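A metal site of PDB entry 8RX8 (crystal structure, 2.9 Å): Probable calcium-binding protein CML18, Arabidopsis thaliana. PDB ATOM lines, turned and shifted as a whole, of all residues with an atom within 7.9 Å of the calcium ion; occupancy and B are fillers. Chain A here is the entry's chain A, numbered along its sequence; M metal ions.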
ATOM      1  N   SER A  35      25.290  -2.465   5.271  1.00  0.00           N
ATOM      2  CA  SER A  35      24.581  -2.583   6.536  1.00  0.00           C
ATOM      3  C   SER A  35      25.487  -3.242   7.558  1.00  0.00           C
ATOM      4  O   SER A  35      26.207  -4.185   7.240  1.00  0.00           O
ATOM      5  CB  SER A  35      23.276  -3.377   6.378  1.00  0.00           C
ATOM      6  OG  SER A  35      23.516  -4.589   5.681  1.00  0.00           O
ATOM      7  N   LEU A  36      25.455  -2.727   8.781  1.00  0.00           N
ATOM      8  CA  LEU A  36      26.275  -3.251   9.866  1.00  0.00           C
ATOM      9  C   LEU A  36      25.512  -4.321  10.640  1.00  0.00           C
ATOM     10  O   LEU A  36      24.310  -4.184  10.886  1.00  0.00           O
ATOM     11  CB  LEU A  36      26.720  -2.129  10.811  1.00  0.00           C
ATOM     12  CG  LEU A  36      28.073  -1.474  10.529  1.00  0.00           C
ATOM     13  CD1 LEU A  36      28.821  -1.239  11.828  1.00  0.00           C
ATOM     14  CD2 LEU A  36      28.917  -2.308   9.566  1.00  0.00           C
ATOM     15  N   ILE A  61      20.712  -1.753  18.557  1.00  0.00           N
ATOM     16  CA  ILE A  61      20.143  -2.249  17.306  1.00  0.00           C
ATOM     17  C   ILE A  61      18.644  -1.955  17.251  1.00  0.00           C
ATOM     18  O   ILE A  61      18.123  -1.482  16.226  1.00  0.00           O
ATOM     19  CB  ILE A  61      20.434  -3.755  17.141  1.00  0.00           C
ATOM     20  CG1 ILE A  61      21.889  -3.963  16.738  1.00  0.00           C
ATOM     21  CG2 ILE A  61      19.492  -4.383  16.127  1.00  0.00           C
ATOM     22  CD1 ILE A  61      22.142  -3.797  15.266  1.00  0.00           C
ATOM     23  N   ALA A  64      17.849   1.601  16.391  1.00  0.00           N
ATOM     24  CA  ALA A  64      18.255   2.110  15.086  1.00  0.00           C
ATOM     25  C   ALA A  64      17.543   1.420  13.942  1.00  0.00           C
ATOM     26  O   ALA A  64      17.121   2.079  12.995  1.00  0.00           O
ATOM     27  CB  ALA A  64      19.765   1.950  14.892  1.00  0.00           C
ATOM     28  N   ASP A  65      17.422   0.100  14.012  1.00  0.00           N
ATOM     29  CA  ASP A  65      16.812  -0.692  12.953  1.00  0.00           C
ATOM     30  C   ASP A  65      15.378  -0.234  12.719  1.00  0.00           C
ATOM     31  O   ASP A  65      14.446  -0.836  13.250  1.00  0.00           O
ATOM     32  CB  ASP A  65      16.873  -2.172  13.326  1.00  0.00           C
ATOM     33  CG  ASP A  65      16.724  -3.088  12.151  1.00  0.00           C
ATOM     34  OD1 ASP A  65      17.281  -2.783  11.084  1.00  0.00           O
ATOM     35  OD2 ASP A  65      16.086  -4.156  12.310  1.00  0.00           O
ATOM     36  N   ARG A  66      15.184   0.820  11.910  1.00  0.00           N
ATOM     37  CA  ARG A  66      13.836   1.332  11.682  1.00  0.00           C
ATOM     38  C   ARG A  66      13.087   0.498  10.658  1.00  0.00           C
ATOM     39  O   ARG A  66      11.868   0.356  10.745  1.00  0.00           O
ATOM     40  CB  ARG A  66      13.864   2.794  11.259  1.00  0.00           C
ATOM     41  CG  ARG A  66      12.534   3.513  11.474  1.00  0.00           C
ATOM     42  CD  ARG A  66      12.540   4.958  10.976  1.00  0.00           C
ATOM     43  NE  ARG A  66      13.836   5.586  11.084  1.00  0.00           N
ATOM     44  CZ  ARG A  66      14.232   6.390  12.072  1.00  0.00           C
ATOM     45  NH1 ARG A  66      14.041   6.061  13.341  1.00  0.00           N
ATOM     46  NH2 ARG A  66      15.022   7.412  11.791  1.00  0.00           N
ATOM     47  N   ASN A  67      13.800  -0.046   9.675  1.00  0.00           N
ATOM     48  CA  ASN A  67      13.189  -0.916   8.679  1.00  0.00           C
ATOM     49  C   ASN A  67      12.948  -2.317   9.216  1.00  0.00           C
ATOM     50  O   ASN A  67      12.399  -3.155   8.501  1.00  0.00           O
ATOM     51  CB  ASN A  67      14.049  -0.968   7.419  1.00  0.00           C
ATOM     52  CG  ASN A  67      15.525  -0.860   7.719  1.00  0.00           C
ATOM     53  OD1 ASN A  67      15.996  -1.343   8.741  1.00  0.00           O
ATOM     54  ND2 ASN A  67      16.263  -0.212   6.821  1.00  0.00           N
ATOM     55  N   ASN A  68      13.342  -2.584  10.468  1.00  0.00           N
ATOM     56  CA  ASN A  68      13.245  -3.912  11.083  1.00  0.00           C
ATOM     57  C   ASN A  68      13.971  -4.964  10.249  1.00  0.00           C
ATOM     58  O   ASN A  68      13.630  -6.147  10.289  1.00  0.00           O
ATOM     59  CB  ASN A  68      11.791  -4.303  11.335  1.00  0.00           C
ATOM     60  CG  ASN A  68      11.014  -3.231  12.110  1.00  0.00           C
ATOM     61  OD1 ASN A  68       9.788  -3.255  12.147  1.00  0.00           O
ATOM     62  ND2 ASN A  68      11.740  -2.325  12.768  1.00  0.00           N
ATOM     63  N   ASN A  69      14.955  -4.514   9.472  1.00  0.00           N
ATOM     64  CA  ASN A  69      15.755  -5.428   8.655  1.00  0.00           C
ATOM     65  C   ASN A  69      16.498  -6.440   9.527  1.00  0.00           C
ATOM     66  O   ASN A  69      16.490  -7.639   9.247  1.00  0.00           O
ATOM     67  CB  ASN A  69      16.775  -4.626   7.837  1.00  0.00           C
ATOM     68  CG  ASN A  69      16.156  -3.953   6.627  1.00  0.00           C
ATOM     69  OD1 ASN A  69      16.809  -3.169   5.939  1.00  0.00           O
ATOM     70  ND2 ASN A  69      14.890  -4.260   6.363  1.00  0.00           N
ATOM     71  N   GLY A  70      17.133  -5.958  10.593  1.00  0.00           N
ATOM     72  CA  GLY A  70      17.984  -6.754  11.446  1.00  0.00           C
ATOM     73  C   GLY A  70      19.425  -6.323  11.376  1.00  0.00           C
ATOM     74  O   GLY A  70      20.250  -6.823  12.160  1.00  0.00           O
ATOM     75  N   LEU A  71      19.745  -5.410  10.480  1.00  0.00           N
ATOM     76  CA  LEU A  71      21.084  -4.863  10.316  1.00  0.00           C
ATOM     77  C   LEU A  71      20.958  -3.348  10.301  1.00  0.00           C
ATOM     78  O   LEU A  71      19.941  -2.802   9.868  1.00  0.00           O
ATOM     79  CB  LEU A  71      21.727  -5.360   9.013  1.00  0.00           C
ATOM     80  CG  LEU A  71      21.879  -6.858   8.807  1.00  0.00           C
ATOM     81  CD1 LEU A  71      22.620  -7.165   7.511  1.00  0.00           C
ATOM     82  CD2 LEU A  71      22.573  -7.504   9.991  1.00  0.00           C
ATOM     83  N   VAL A  72      21.998  -2.665  10.767  1.00  0.00           N
ATOM     84  CA  VAL A  72      21.984  -1.207  10.838  1.00  0.00           C
ATOM     85  C   VAL A  72      22.616  -0.645   9.569  1.00  0.00           C
ATOM     86  O   VAL A  72      23.776  -0.952   9.259  1.00  0.00           O
ATOM     87  CB  VAL A  72      22.688  -0.679  12.095  1.00  0.00           C
ATOM     88  CG1 VAL A  72      23.657  -1.715  12.656  1.00  0.00           C
ATOM     89  CG2 VAL A  72      23.373   0.662  11.830  1.00  0.00           C
ATOM     90  N   GLU A  73      21.853   0.137   8.829  1.00  0.00           N
ATOM     91  CA  GLU A  73      22.307   0.747   7.592  1.00  0.00           C
ATOM     92  C   GLU A  73      22.824   2.145   7.895  1.00  0.00           C
ATOM     93  O   GLU A  73      22.614   2.687   8.977  1.00  0.00           O
ATOM     94  CB  GLU A  73      21.182   0.772   6.562  1.00  0.00           C
ATOM     95  CG  GLU A  73      20.884  -0.595   5.952  1.00  0.00           C
ATOM     96  CD  GLU A  73      19.917  -1.403   6.804  1.00  0.00           C
ATOM     97  OE1 GLU A  73      18.980  -0.807   7.365  1.00  0.00           O
ATOM     98  OE2 GLU A  73      20.095  -2.634   6.905  1.00  0.00           O
ATOM     99  N   PHE A  74      23.545   2.731   6.922  1.00  0.00           N
ATOM    100  CA  PHE A  74      24.169   4.032   7.176  1.00  0.00           C
ATOM    101  C   PHE A  74      23.140   5.076   7.573  1.00  0.00           C
ATOM    102  O   PHE A  74      23.406   5.921   8.439  1.00  0.00           O
ATOM    103  CB  PHE A  74      24.957   4.489   5.957  1.00  0.00           C
ATOM    104  CG  PHE A  74      25.806   5.690   6.213  1.00  0.00           C
ATOM    105  CD1 PHE A  74      26.771   5.671   7.205  1.00  0.00           C
ATOM    106  CD2 PHE A  74      25.637   6.851   5.480  1.00  0.00           C
ATOM    107  CE1 PHE A  74      27.546   6.784   7.455  1.00  0.00           C
ATOM    108  CE2 PHE A  74      26.414   7.961   5.712  1.00  0.00           C
ATOM    109  CZ  PHE A  74      27.378   7.927   6.712  1.00  0.00           C
ATOM    110  N   SER A  75      21.956   5.036   6.961  1.00  0.00           N
ATOM    111  CA  SER A  75      20.914   6.002   7.314  1.00  0.00           C
ATOM    112  C   SER A  75      20.498   5.830   8.773  1.00  0.00           C
ATOM    113  O   SER A  75      20.349   6.826   9.493  1.00  0.00           O
ATOM    114  CB  SER A  75      19.703   5.846   6.388  1.00  0.00           C
ATOM    115  OG  SER A  75      19.361   4.488   6.205  1.00  0.00           O
ATOM    116  N   GLU A  76      20.312   4.588   9.225  1.00  0.00           N
ATOM    117  CA  GLU A  76      19.936   4.351  10.614  1.00  0.00           C
ATOM    118  C   GLU A  76      21.035   4.815  11.556  1.00  0.00           C
ATOM    119  O   GLU A  76      20.767   5.343  12.640  1.00  0.00           O
ATOM    120  CB  GLU A  76      19.656   2.866  10.820  1.00  0.00           C
ATOM    121  CG  GLU A  76      19.078   2.167   9.588  1.00  0.00           C
ATOM    122  CD  GLU A  76      18.263   0.931   9.929  1.00  0.00           C
ATOM    123  OE1 GLU A  76      18.876  -0.131  10.149  1.00  0.00           O
ATOM    124  OE2 GLU A  76      17.019   1.028   9.972  1.00  0.00           O
ATOM    125  N   GLU A 137       9.489  -3.251   5.723  1.00  0.00           N
ATOM    126  CA  GLU A 137      10.551  -2.266   5.901  1.00  0.00           C
ATOM    127  C   GLU A 137      10.004  -0.844   6.027  1.00  0.00           C
ATOM    128  O   GLU A 137      10.453  -0.083   6.884  1.00  0.00           O
ATOM    129  CB  GLU A 137      11.549  -2.367   4.735  1.00  0.00           C
ATOM    130  CG  GLU A 137      12.196  -1.063   4.325  1.00  0.00           C
ATOM    131  CD  GLU A 137      12.958  -1.191   3.014  1.00  0.00           C
ATOM    132  OE1 GLU A 137      13.272  -2.343   2.631  1.00  0.00           O
ATOM    133  OE2 GLU A 137      13.232  -0.154   2.373  1.00  0.00           O
ATOM    134  N   SER A 157      15.072   7.715   3.903  1.00  0.00           N
ATOM    135  CA  SER A 157      16.092   6.784   4.397  1.00  0.00           C
ATOM    136  C   SER A 157      16.815   6.096   3.241  1.00  0.00           C
ATOM    137  O   SER A 157      18.030   5.858   3.312  1.00  0.00           O
ATOM    138  CB  SER A 157      15.459   5.754   5.334  1.00  0.00           C
ATOM    139  OG  SER A 157      16.435   4.888   5.874  1.00  0.00           O
HETATM  140 CA    CA M   1      18.030  -1.927   9.139  1.00  0.00          CA
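The calcium ion is bound by OD1 of Asn 67 (2.2 Å), O of Leu 71 (2.2 Å), OE1 of Glu 76 (2.2 Å), OD1 of Asp 65 (2.3 Å) and OE1 of Glu 73 (2.3 Å). Slightly farther from the calcium ion lies OE2 of Glu 73 (3.1 Å).
Merely in contact with the calcium ion: Asn 69. Within 4 Å of the calcium ion: Asp 65, Asn 67, Asn 69, Leu 71, Glu 73 and Glu 76. The nearest printed residue that does not touch the calcium ion is Val 72 (4.4 Å).
The side-chain amide oxygen (OD1) of Asn 69 sits at hydrogen-bond distance from the side-chain amide nitrogen (ND2) of Asn 67, 3.1 Å away. The side-chain carboxylate of Glu 76 is in hydrogen-bond range of the backbone NH of Arg 66. The side-chain carboxylate of Asp 65 is in hydrogen-bond range of the backbone NH of Asn 69 (3.1 Å). OD2 of Asp 65 sits at hydrogen-bond distance from N of Gly 70 (2.7 Å). O of Asp 65 lies within hydrogen-bond range of ND2 of Asn 68 (3.1 Å). OD1 of Asn 69 lies close to OE2 of Glu 73, 3.5 Å away.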
